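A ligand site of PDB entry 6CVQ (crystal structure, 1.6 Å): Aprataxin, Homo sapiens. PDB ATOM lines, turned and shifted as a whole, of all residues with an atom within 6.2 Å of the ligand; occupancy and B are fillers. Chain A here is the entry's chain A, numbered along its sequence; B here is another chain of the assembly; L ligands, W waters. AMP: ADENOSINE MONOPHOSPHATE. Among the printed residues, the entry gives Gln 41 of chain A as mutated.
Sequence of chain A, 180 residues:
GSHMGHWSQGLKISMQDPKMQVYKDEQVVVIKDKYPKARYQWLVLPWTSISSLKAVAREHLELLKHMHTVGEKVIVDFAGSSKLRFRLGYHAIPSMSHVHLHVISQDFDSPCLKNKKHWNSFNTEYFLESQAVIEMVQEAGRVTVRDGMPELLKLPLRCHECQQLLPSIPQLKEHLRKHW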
ATOM      1  N   TRP A   7      26.607 -22.740 -24.089  1.00  0.00           N
ATOM      2  CA  TRP A   7      25.518 -21.759 -24.120  1.00  0.00           C
ATOM      3  C   TRP A   7      25.355 -21.044 -22.793  1.00  0.00           C
ATOM      4  O   TRP A   7      24.989 -19.867 -22.770  1.00  0.00           O
ATOM      5  CB  TRP A   7      24.194 -22.434 -24.540  1.00  0.00           C
ATOM      6  CG  TRP A   7      23.656 -23.469 -23.570  1.00  0.00           C
ATOM      7  CD1 TRP A   7      23.739 -24.835 -23.691  1.00  0.00           C
ATOM      8  CD2 TRP A   7      22.923 -23.221 -22.368  1.00  0.00           C
ATOM      9  NE1 TRP A   7      23.117 -25.442 -22.630  1.00  0.00           N
ATOM     10  CE2 TRP A   7      22.618 -24.479 -21.795  1.00  0.00           C
ATOM     11  CE3 TRP A   7      22.510 -22.068 -21.691  1.00  0.00           C
ATOM     12  CZ2 TRP A   7      21.926 -24.604 -20.584  1.00  0.00           C
ATOM     13  CZ3 TRP A   7      21.818 -22.193 -20.480  1.00  0.00           C
ATOM     14  CH2 TRP A   7      21.540 -23.449 -19.943  1.00  0.00           C
ATOM     15  N   GLY A  10      27.071 -17.452 -22.213  1.00  0.00           N
ATOM     16  CA  GLY A  10      26.866 -16.400 -23.202  1.00  0.00           C
ATOM     17  C   GLY A  10      26.845 -14.984 -22.656  1.00  0.00           C
ATOM     18  O   GLY A  10      27.178 -14.045 -23.360  1.00  0.00           O
ATOM     19  N   LEU A  11      26.389 -14.802 -21.414  1.00  0.00           N
ATOM     20  CA  LEU A  11      26.395 -13.463 -20.835  1.00  0.00           C
ATOM     21  C   LEU A  11      27.820 -12.952 -20.644  1.00  0.00           C
ATOM     22  O   LEU A  11      28.059 -11.740 -20.709  1.00  0.00           O
ATOM     23  CB  LEU A  11      25.670 -13.434 -19.501  1.00  0.00           C
ATOM     24  CG  LEU A  11      24.208 -13.860 -19.511  1.00  0.00           C
ATOM     25  CD1 LEU A  11      23.588 -13.670 -18.135  1.00  0.00           C
ATOM     26  CD2 LEU A  11      23.413 -13.116 -20.550  1.00  0.00           C
ATOM     27  N   SER A  14      28.517 -11.418 -23.994  1.00  0.00           N
ATOM     28  CA  SER A  14      27.714 -10.244 -24.311  1.00  0.00           C
ATOM     29  C   SER A  14      28.071  -9.049 -23.441  1.00  0.00           C
ATOM     30  O   SER A  14      28.069  -7.907 -23.915  1.00  0.00           O
ATOM     31  CB  SER A  14      26.233 -10.572 -24.146  1.00  0.00           C
ATOM     32  OG  SER A  14      25.862 -11.509 -25.132  1.00  0.00           O
ATOM     33  N   MET A  20      26.078  -4.140 -27.237  1.00  0.00           N
ATOM     34  CA  MET A  20      25.033  -4.559 -26.316  1.00  0.00           C
ATOM     35  C   MET A  20      25.079  -3.791 -25.004  1.00  0.00           C
ATOM     36  O   MET A  20      24.100  -3.829 -24.247  1.00  0.00           O
ATOM     37  CB  MET A  20      25.154  -6.056 -26.065  1.00  0.00           C
ATOM     38  CG  MET A  20      24.958  -6.906 -27.345  1.00  0.00           C
ATOM     39  SD  MET A  20      25.037  -8.618 -26.814  1.00  0.00           S
ATOM     40  CE  MET A  20      24.876  -9.484 -28.392  1.00  0.00           C
ATOM     41  N   ILE A  31      23.492  -4.529 -20.092  1.00  0.00           N
ATOM     42  CA  ILE A  31      23.292  -4.923 -21.479  1.00  0.00           C
ATOM     43  C   ILE A  31      21.807  -5.093 -21.742  1.00  0.00           C
ATOM     44  O   ILE A  31      20.998  -5.328 -20.845  1.00  0.00           O
ATOM     45  CB  ILE A  31      24.051  -6.223 -21.841  1.00  0.00           C
ATOM     46  CG1 ILE A  31      23.562  -7.408 -20.997  1.00  0.00           C
ATOM     47  CG2 ILE A  31      25.555  -6.020 -21.713  1.00  0.00           C
ATOM     48  CD1 ILE A  31      24.174  -8.765 -21.443  1.00  0.00           C
ATOM     49  N   LYS A  32      21.460  -4.991 -23.024  1.00  0.00           N
ATOM     50  CA  LYS A  32      20.129  -5.383 -23.463  1.00  0.00           C
ATOM     51  C   LYS A  32      20.000  -6.898 -23.402  1.00  0.00           C
ATOM     52  O   LYS A  32      20.902  -7.643 -23.794  1.00  0.00           O
ATOM     53  CB  LYS A  32      19.882  -4.883 -24.883  1.00  0.00           C
ATOM     54  CG  LYS A  32      19.883  -3.362 -25.009  1.00  0.00           C
ATOM     55  CD  LYS A  32      20.301  -2.883 -26.407  1.00  0.00           C
ATOM     56  CE  LYS A  32      19.353  -3.354 -27.478  1.00  0.00           C
ATOM     57  NZ  LYS A  32      19.775  -2.857 -28.844  1.00  0.00           N
ATOM     58  N   ASP A  33      18.876  -7.378 -22.886  1.00  0.00           N
ATOM     59  CA  ASP A  33      18.565  -8.799 -22.999  1.00  0.00           C
ATOM     60  C   ASP A  33      18.470  -9.189 -24.474  1.00  0.00           C
ATOM     61  O   ASP A  33      17.838  -8.492 -25.271  1.00  0.00           O
ATOM     62  CB  ASP A  33      17.261  -9.094 -22.281  1.00  0.00           C
ATOM     63  CG  ASP A  33      17.092 -10.572 -21.976  1.00  0.00           C
ATOM     64  OD1 ASP A  33      16.863 -11.351 -22.920  1.00  0.00           O
ATOM     65  OD2 ASP A  33      17.188 -10.954 -20.801  1.00  0.00           O
ATOM     66  N   LYS A  34      19.084 -10.314 -24.828  1.00  0.00           N
ATOM     67  CA  LYS A  34      19.112 -10.748 -26.222  1.00  0.00           C
ATOM     68  C   LYS A  34      17.754 -11.238 -26.694  1.00  0.00           C
ATOM     69  O   LYS A  34      17.441 -11.170 -27.896  1.00  0.00           O
ATOM     70  CB  LYS A  34      20.172 -11.845 -26.375  1.00  0.00           C
ATOM     71  CG  LYS A  34      20.409 -12.283 -27.795  1.00  0.00           C
ATOM     72  CD  LYS A  34      21.573 -13.233 -27.873  1.00  0.00           C
ATOM     73  CE  LYS A  34      21.798 -13.701 -29.299  1.00  0.00           C
ATOM     74  NZ  LYS A  34      22.979 -14.547 -29.380  1.00  0.00           N
ATOM     75  N   TYR A  35      16.938 -11.716 -25.769  1.00  0.00           N
ATOM     76  CA  TYR A  35      15.636 -12.311 -26.070  1.00  0.00           C
ATOM     77  C   TYR A  35      14.597 -11.682 -25.157  1.00  0.00           C
ATOM     78  O   TYR A  35      14.010 -12.352 -24.318  1.00  0.00           O
ATOM     79  CB  TYR A  35      15.682 -13.822 -25.889  1.00  0.00           C
ATOM     80  CG  TYR A  35      16.766 -14.509 -26.674  1.00  0.00           C
ATOM     81  CD1 TYR A  35      16.631 -14.743 -28.033  1.00  0.00           C
ATOM     82  CD2 TYR A  35      17.924 -14.958 -26.053  1.00  0.00           C
ATOM     83  CE1 TYR A  35      17.611 -15.406 -28.744  1.00  0.00           C
ATOM     84  CE2 TYR A  35      18.906 -15.582 -26.742  1.00  0.00           C
ATOM     85  CZ  TYR A  35      18.749 -15.817 -28.089  1.00  0.00           C
ATOM     86  OH  TYR A  35      19.769 -16.469 -28.751  1.00  0.00           O
ATOM     87  N   PRO A  36      14.377 -10.379 -25.283  1.00  0.00           N
ATOM     88  CA  PRO A  36      13.591  -9.682 -24.272  1.00  0.00           C
ATOM     89  C   PRO A  36      12.156 -10.211 -24.222  1.00  0.00           C
ATOM     90  O   PRO A  36      11.546 -10.494 -25.250  1.00  0.00           O
ATOM     91  CB  PRO A  36      13.647  -8.215 -24.728  1.00  0.00           C
ATOM     92  CG  PRO A  36      13.889  -8.287 -26.201  1.00  0.00           C
ATOM     93  CD  PRO A  36      14.780  -9.497 -26.386  1.00  0.00           C
ATOM     94  N   LYS A  37      11.648 -10.356 -23.006  1.00  0.00           N
ATOM     95  CA  LYS A  37      10.298 -10.857 -22.780  1.00  0.00           C
ATOM     96  C   LYS A  37       9.285  -9.731 -22.582  1.00  0.00           C
ATOM     97  O   LYS A  37       8.122  -9.997 -22.257  1.00  0.00           O
ATOM     98  CB  LYS A  37      10.295 -11.800 -21.581  1.00  0.00           C
ATOM     99  CG  LYS A  37      11.324 -12.956 -21.672  1.00  0.00           C
ATOM    100  CD  LYS A  37      11.179 -13.762 -22.927  1.00  0.00           C
ATOM    101  CE  LYS A  37      12.089 -15.011 -22.947  1.00  0.00           C
ATOM    102  NZ  LYS A  37      13.556 -14.726 -22.887  1.00  0.00           N
ATOM    103  N   GLN A  41      13.866  -4.779 -21.561  1.00  0.00           N
ATOM    104  CA  GLN A  41      14.496  -5.716 -20.641  1.00  0.00           C
ATOM    105  C   GLN A  41      15.999  -5.535 -20.715  1.00  0.00           C
ATOM    106  O   GLN A  41      16.614  -5.693 -21.780  1.00  0.00           O
ATOM    107  CB  GLN A  41      14.122  -7.166 -20.942  1.00  0.00           C
ATOM    108  CG  GLN A  41      14.590  -8.118 -19.848  1.00  0.00           C
ATOM    109  CD  GLN A  41      14.132  -9.557 -20.054  1.00  0.00           C
ATOM    110  OE1 GLN A  41      13.511  -9.879 -21.042  1.00  0.00           O
ATOM    111  NE2 GLN A  41      14.412 -10.424 -19.095  1.00  0.00           N
ATOM    112  N   LEU A  43      19.789  -6.422 -18.432  1.00  0.00           N
ATOM    113  CA  LEU A  43      20.506  -7.180 -17.426  1.00  0.00           C
ATOM    114  C   LEU A  43      21.638  -6.334 -16.872  1.00  0.00           C
ATOM    115  O   LEU A  43      22.435  -5.775 -17.641  1.00  0.00           O
ATOM    116  CB  LEU A  43      21.071  -8.476 -18.030  1.00  0.00           C
ATOM    117  CG  LEU A  43      20.042  -9.339 -18.756  1.00  0.00           C
ATOM    118  CD1 LEU A  43      20.718 -10.564 -19.359  1.00  0.00           C
ATOM    119  CD2 LEU A  43      18.934  -9.771 -17.805  1.00  0.00           C
ATOM    120  N   HIS A  91      15.768 -14.540 -11.169  1.00  0.00           N
ATOM    121  CA  HIS A  91      15.110 -15.839 -11.203  1.00  0.00           C
ATOM    122  C   HIS A  91      15.634 -16.716 -10.084  1.00  0.00           C
ATOM    123  O   HIS A  91      16.833 -16.742  -9.784  1.00  0.00           O
ATOM    124  CB  HIS A  91      15.329 -16.524 -12.546  1.00  0.00           C
ATOM    125  CG  HIS A  91      14.509 -15.942 -13.650  1.00  0.00           C
ATOM    126  ND1 HIS A  91      14.878 -16.029 -14.976  1.00  0.00           N
ATOM    127  CD2 HIS A  91      13.341 -15.260 -13.634  1.00  0.00           C
ATOM    128  CE1 HIS A  91      13.964 -15.426 -15.721  1.00  0.00           C
ATOM    129  NE2 HIS A  91      13.022 -14.964 -14.932  1.00  0.00           N
ATOM    130  N   ILE A  93      15.993 -19.848  -9.892  1.00  0.00           N
ATOM    131  CA  ILE A  93      16.973 -20.769 -10.469  1.00  0.00           C
ATOM    132  C   ILE A  93      17.321 -20.204 -11.842  1.00  0.00           C
ATOM    133  O   ILE A  93      16.507 -20.311 -12.771  1.00  0.00           O
ATOM    134  CB  ILE A  93      16.410 -22.199 -10.620  1.00  0.00           C
ATOM    135  CG1 ILE A  93      15.905 -22.713  -9.263  1.00  0.00           C
ATOM    136  CG2 ILE A  93      17.472 -23.126 -11.190  1.00  0.00           C
ATOM    137  CD1 ILE A  93      15.262 -24.074  -9.346  1.00  0.00           C
ATOM    138  N   PRO A  94      18.477 -19.603 -12.029  1.00  0.00           N
ATOM    139  CA  PRO A  94      18.839 -19.094 -13.349  1.00  0.00           C
ATOM    140  C   PRO A  94      19.326 -20.225 -14.251  1.00  0.00           C
ATOM    141  O   PRO A  94      19.623 -21.342 -13.825  1.00  0.00           O
ATOM    142  CB  PRO A  94      19.966 -18.107 -13.043  1.00  0.00           C
ATOM    143  CG  PRO A  94      20.636 -18.709 -11.847  1.00  0.00           C
ATOM    144  CD  PRO A  94      19.541 -19.360 -11.038  1.00  0.00           C
ATOM    145  N   SER A  95      19.399 -19.902 -15.543  1.00  0.00           N
ATOM    146  CA  SER A  95      20.016 -20.766 -16.546  1.00  0.00           C
ATOM    147  C   SER A  95      21.408 -20.297 -16.950  1.00  0.00           C
ATOM    148  O   SER A  95      22.313 -21.132 -17.148  1.00  0.00           O
ATOM    149  CB  SER A  95      19.135 -20.815 -17.789  1.00  0.00           C
ATOM    150  OG  SER A  95      17.881 -21.406 -17.490  1.00  0.00           O
ATOM    151  N   MET A  96      21.605 -18.999 -17.076  1.00  0.00           N
ATOM    152  CA  MET A  96      22.860 -18.433 -17.547  1.00  0.00           C
ATOM    153  C   MET A  96      23.786 -18.126 -16.380  1.00  0.00           C
ATOM    154  O   MET A  96      23.347 -17.581 -15.354  1.00  0.00           O
ATOM    155  CB  MET A  96      22.599 -17.153 -18.336  1.00  0.00           C
ATOM    156  CG  MET A  96      21.676 -17.320 -19.547  1.00  0.00           C
ATOM    157  SD  MET A  96      22.417 -18.355 -20.811  1.00  0.00           S
ATOM    158  CE  MET A  96      23.675 -17.265 -21.484  1.00  0.00           C
ATOM    159  N   SER A  97      25.060 -18.448 -16.548  1.00  0.00           N
ATOM    160  CA  SER A  97      26.076 -18.154 -15.551  1.00  0.00           C
ATOM    161  C   SER A  97      26.371 -16.663 -15.485  1.00  0.00           C
ATOM    162  O   SER A  97      26.162 -15.907 -16.443  1.00  0.00           O
ATOM    163  CB  SER A  97      27.379 -18.889 -15.869  1.00  0.00           C
ATOM    164  OG  SER A  97      27.181 -20.282 -15.892  1.00  0.00           O
ATOM    165  N   HIS A 100      23.246 -11.797 -12.513  1.00  0.00           N
ATOM    166  CA  HIS A 100      22.662 -10.736 -13.320  1.00  0.00           C
ATOM    167  C   HIS A 100      21.294 -10.376 -12.773  1.00  0.00           C
ATOM    168  O   HIS A 100      20.510 -11.255 -12.397  1.00  0.00           O
ATOM    169  CB  HIS A 100      22.565 -11.155 -14.780  1.00  0.00           C
ATOM    170  CG  HIS A 100      21.892 -12.476 -14.997  1.00  0.00           C
ATOM    171  ND1 HIS A 100      22.549 -13.679 -14.859  1.00  0.00           N
ATOM    172  CD2 HIS A 100      20.632 -12.779 -15.380  1.00  0.00           C
ATOM    173  CE1 HIS A 100      21.716 -14.671 -15.119  1.00  0.00           C
ATOM    174  NE2 HIS A 100      20.554 -14.142 -15.455  1.00  0.00           N
ATOM    175  N   HIS A 102      17.688  -8.744 -13.531  1.00  0.00           N
ATOM    176  CA  HIS A 102      16.695  -8.403 -14.537  1.00  0.00           C
ATOM    177  C   HIS A 102      16.029  -7.069 -14.208  1.00  0.00           C
ATOM    178  O   HIS A 102      15.621  -6.833 -13.067  1.00  0.00           O
ATOM    179  CB  HIS A 102      15.609  -9.474 -14.614  1.00  0.00           C
ATOM    180  CG  HIS A 102      16.045 -10.736 -15.258  1.00  0.00           C
ATOM    181  ND1 HIS A 102      15.868 -10.984 -16.599  1.00  0.00           N
ATOM    182  CD2 HIS A 102      16.652 -11.828 -14.737  1.00  0.00           C
ATOM    183  CE1 HIS A 102      16.354 -12.186 -16.883  1.00  0.00           C
ATOM    184  NE2 HIS A 102      16.828 -12.718 -15.765  1.00  0.00           N
ATOM    185  N   PHE A 122       8.589 -14.860 -14.572  1.00  0.00           N
ATOM    186  CA  PHE A 122       8.506 -13.450 -14.210  1.00  0.00           C
ATOM    187  C   PHE A 122       7.272 -13.078 -13.405  1.00  0.00           C
ATOM    188  O   PHE A 122       7.225 -11.961 -12.866  1.00  0.00           O
ATOM    189  CB  PHE A 122       8.565 -12.579 -15.479  1.00  0.00           C
ATOM    190  CG  PHE A 122       9.897 -12.598 -16.147  1.00  0.00           C
ATOM    191  CD1 PHE A 122      10.937 -11.835 -15.653  1.00  0.00           C
ATOM    192  CD2 PHE A 122      10.135 -13.408 -17.241  1.00  0.00           C
ATOM    193  CE1 PHE A 122      12.186 -11.853 -16.261  1.00  0.00           C
ATOM    194  CE2 PHE A 122      11.370 -13.443 -17.850  1.00  0.00           C
ATOM    195  CZ  PHE A 122      12.407 -12.667 -17.351  1.00  0.00           C
ATOM    196  N   TYR A 126       8.823 -17.397  -8.423  1.00  0.00           N
ATOM    197  CA  TYR A 126      10.092 -17.727  -9.067  1.00  0.00           C
ATOM    198  C   TYR A 126      10.897 -16.468  -9.348  1.00  0.00           C
ATOM    199  O   TYR A 126      12.123 -16.538  -9.456  1.00  0.00           O
ATOM    200  CB  TYR A 126       9.790 -18.468 -10.370  1.00  0.00           C
ATOM    201  CG  TYR A 126      10.899 -19.287 -10.965  1.00  0.00           C
ATOM    202  CD1 TYR A 126      11.816 -18.722 -11.839  1.00  0.00           C
ATOM    203  CD2 TYR A 126      10.987 -20.632 -10.723  1.00  0.00           C
ATOM    204  CE1 TYR A 126      12.796 -19.496 -12.439  1.00  0.00           C
ATOM    205  CE2 TYR A 126      11.954 -21.408 -11.305  1.00  0.00           C
ATOM    206  CZ  TYR A 126      12.847 -20.830 -12.163  1.00  0.00           C
ATOM    207  OH  TYR A 126      13.804 -21.633 -12.738  1.00  0.00           O
ATOM    208  OP3   G B   1      13.571 -19.607 -20.840  1.00  0.00           O
ATOM    209  P     G B   1      14.474 -20.312 -19.720  1.00  0.00           P
ATOM    210  OP1   G B   1      14.348 -21.785 -19.903  1.00  0.00           O
ATOM    211  OP2   G B   1      14.126 -19.692 -18.419  1.00  0.00           O
ATOM    212  O5'   G B   1      15.978 -19.990 -20.117  1.00  0.00           O
ATOM    213  C5'   G B   1      16.481 -18.650 -20.054  1.00  0.00           C
ATOM    214  C4'   G B   1      17.448 -18.433 -21.176  1.00  0.00           C
ATOM    215  O4'   G B   1      18.613 -19.256 -20.950  1.00  0.00           O
ATOM    216  C3'   G B   1      16.948 -18.859 -22.542  1.00  0.00           C
ATOM    217  O3'   G B   1      16.176 -17.861 -23.181  1.00  0.00           O
ATOM    218  C2'   G B   1      18.223 -19.205 -23.279  1.00  0.00           C
ATOM    219  O2'   G B   1      18.927 -18.046 -23.696  1.00  0.00           O
ATOM    220  C1'   G B   1      19.023 -19.841 -22.160  1.00  0.00           C
ATOM    221  N9    G B   1      18.867 -21.308 -22.037  1.00  0.00           N
ATOM    222  C8    G B   1      18.318 -21.999 -20.988  1.00  0.00           C
ATOM    223  N7    G B   1      18.399 -23.305 -21.128  1.00  0.00           N
ATOM    224  C5    G B   1      19.059 -23.462 -22.335  1.00  0.00           C
ATOM    225  C6    G B   1      19.451 -24.650 -23.008  1.00  0.00           C
ATOM    226  O6    G B   1      19.301 -25.831 -22.672  1.00  0.00           O
ATOM    227  N1    G B   1      20.091 -24.370 -24.203  1.00  0.00           N
ATOM    228  C2    G B   1      20.339 -23.110 -24.684  1.00  0.00           C
ATOM    229  N2    G B   1      20.980 -23.067 -25.862  1.00  0.00           N
ATOM    230  N3    G B   1      19.997 -21.990 -24.074  1.00  0.00           N
ATOM    231  C4    G B   1      19.345 -22.252 -22.909  1.00  0.00           C
ATOM    232  P    DT B   2      14.903 -18.263 -24.063  1.00  0.00           P
ATOM    233  OP1  DT B   2      14.286 -16.975 -24.402  1.00  0.00           O
ATOM    234  OP2  DT B   2      14.113 -19.324 -23.399  1.00  0.00           O
ATOM    235  O5'  DT B   2      15.530 -18.930 -25.372  1.00  0.00           O
ATOM    236  C5'  DT B   2      16.417 -18.179 -26.205  1.00  0.00           C
ATOM    237  C4'  DT B   2      17.032 -19.068 -27.262  1.00  0.00           C
ATOM    238  O4'  DT B   2      17.833 -20.074 -26.611  1.00  0.00           O
ATOM    239  C3'  DT B   2      16.051 -19.845 -28.132  1.00  0.00           C
ATOM    240  O3'  DT B   2      15.646 -19.080 -29.229  1.00  0.00           O
ATOM    241  C2'  DT B   2      16.851 -21.041 -28.545  1.00  0.00           C
ATOM    242  C1'  DT B   2      17.751 -21.280 -27.364  1.00  0.00           C
ATOM    243  N1   DT B   2      17.302 -22.372 -26.489  1.00  0.00           N
ATOM    244  C2   DT B   2      17.643 -23.646 -26.862  1.00  0.00           C
ATOM    245  O2   DT B   2      18.240 -23.878 -27.901  1.00  0.00           O
ATOM    246  N3   DT B   2      17.232 -24.628 -26.017  1.00  0.00           N
ATOM    247  C4   DT B   2      16.537 -24.475 -24.832  1.00  0.00           C
ATOM    248  O4   DT B   2      16.238 -25.425 -24.125  1.00  0.00           O
ATOM    249  C5   DT B   2      16.200 -23.102 -24.494  1.00  0.00           C
ATOM    250  C7   DT B   2      15.446 -22.810 -23.238  1.00  0.00           C
ATOM    251  C6   DT B   2      16.594 -22.124 -25.336  1.00  0.00           C
HETATM  252  P   AMP L   1      18.121 -16.479 -16.466  1.00  0.00           P
HETATM  253  O1P AMP L   1      16.898 -17.254 -16.077  1.00  0.00           O
HETATM  254  O2P AMP L   1      18.140 -15.188 -15.682  1.00  0.00           O
HETATM  255  O3P AMP L   1      19.380 -17.260 -16.487  1.00  0.00           O
HETATM  256  O5' AMP L   1      17.820 -16.092 -17.970  1.00  0.00           O
HETATM  257  C5' AMP L   1      18.849 -15.617 -18.826  1.00  0.00           C
HETATM  258  C4' AMP L   1      18.457 -14.322 -19.490  1.00  0.00           C
HETATM  259  O4' AMP L   1      19.494 -13.944 -20.409  1.00  0.00           O
HETATM  260  C3' AMP L   1      17.161 -14.405 -20.315  1.00  0.00           C
HETATM  261  O3' AMP L   1      16.362 -13.260 -20.046  1.00  0.00           O
HETATM  262  C2' AMP L   1      17.660 -14.430 -21.766  1.00  0.00           C
HETATM  263  O2' AMP L   1      16.788 -13.855 -22.719  1.00  0.00           O
HETATM  264  C1' AMP L   1      18.963 -13.653 -21.679  1.00  0.00           C
HETATM  265  N9  AMP L   1      20.026 -14.032 -22.611  1.00  0.00           N
HETATM  266  C8  AMP L   1      20.400 -15.250 -23.017  1.00  0.00           C
HETATM  267  N7  AMP L   1      21.506 -15.227 -23.745  1.00  0.00           N
HETATM  268  C5  AMP L   1      21.884 -13.889 -23.767  1.00  0.00           C
HETATM  269  C6  AMP L   1      22.956 -13.210 -24.343  1.00  0.00           C
HETATM  270  N6  AMP L   1      23.887 -13.836 -25.066  1.00  0.00           N
HETATM  271  N1  AMP L   1      23.040 -11.865 -24.162  1.00  0.00           N
HETATM  272  C2  AMP L   1      22.097 -11.246 -23.442  1.00  0.00           C
HETATM  273  N3  AMP L   1      21.037 -11.802 -22.843  1.00  0.00           N
HETATM  274  C4  AMP L   1      20.975 -13.147 -23.035  1.00  0.00           C
HETATM  275  O   HOH W   1      16.053 -19.697 -16.532  1.00  0.00           O
HETATM  276  O   HOH W   2      18.009 -14.533 -12.968  1.00  0.00           O
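The side-chain hydroxyl (OG) of Ser 14 lies within hydrogen-bond range of the side-chain sulfur (SD) of Met 20 (3.4 Å).
The side-chain amino group (NZ) of Lys 37 is in salt-bridge range of OP1 of DT 2 of chain B, at 2.8 Å.
The backbone NH (N) of Lys 32 is in hydrogen-bond range of the backbone carbonyl oxygen (O) of Met 20, 3.1 Å away.
The backbone NH of Leu 43 is in hydrogen-bond range of the backbone carbonyl oxygen of Ile 31 (2.9 Å).
The side-chain amide nitrogen (NE2) of Gln 41 lies within hydrogen-bond range of a ring nitrogen (ND1) of His 102.
O of Gly 10 is in hydrogen-bond range of OG of Ser 14, at 3.4 Å.
NZ of Lys 37 lies within hydrogen-bond range of O of Tyr 35.
The backbone NH of Asp 33 lies within hydrogen-bond range of the backbone carbonyl oxygen of Gln 41 (3.0 Å).
Water W1 lies within hydrogen-bond range of an oxygen (O1P) of the ligand (2.6 Å), the side-chain hydroxyl of Ser 95 (2.7 Å) and OP2 of G 1 of chain B (2.7 Å).
Water W2 lies within hydrogen-bond range of O2P of the ligand (2.8 Å) and N of His 91 (2.9 Å).
Gly 10 touches the ligand (O to N6, 3.7 Å).
CD2 of Leu 11 touches C4 of the ligand, 3.5 Å away.
CD1 of Ile 31 touches C2 of the ligand (3.8 Å).
O of Lys 32 touches C2 of the ligand (3.8 Å).
CB of Tyr 35 touches O2' of the ligand, at 3.4 Å.
Gln 41 touches the ligand.
Leu 43 touches the ligand.
Pro 94 touches the ligand.
G 1 of chain B touches the ligand (O2' to C8, 3.2 Å).
Within 4 Å of the ligand: Gly 10, Leu 11, Ser 14, Ile 31, Lys 32, Asp 33, Lys 34, Tyr 35, Lys 37, Gln 41, Leu 43, His 91, Pro 94, Ser 95, Met 96, His 100, His 102 and G 1 of chain B.
The side-chain carboxylate (OD1) of Asp 33 sits at hydrogen-bond distance from an oxygen (O2') of the ligand (2.5 Å).
An oxygen (O2P) of the ligand lies within hydrogen-bond range of a ring nitrogen (NE2) of His 102.
An oxygen (O3P) of the ligand is in hydrogen-bond range of the backbone NH (N) of Ser 95 (2.8 Å).
OG of Ser 14 lies within hydrogen-bond range of N1 of the ligand, 3.0 Å away.
O1P of the ligand is in hydrogen-bond range of ND1 of His 91.
N3 of the ligand lies within hydrogen-bond range of N of Lys 34, at 3.2 Å.
The side-chain amino group (NZ) of Lys 37 sits at hydrogen-bond distance from an oxygen (O2') of the ligand (3.4 Å).
NE2 of His 100 is in hydrogen-bond range of O2P of the ligand.
O3P of the ligand is in hydrogen-bond range of N of Met 96, 2.9 Å away.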
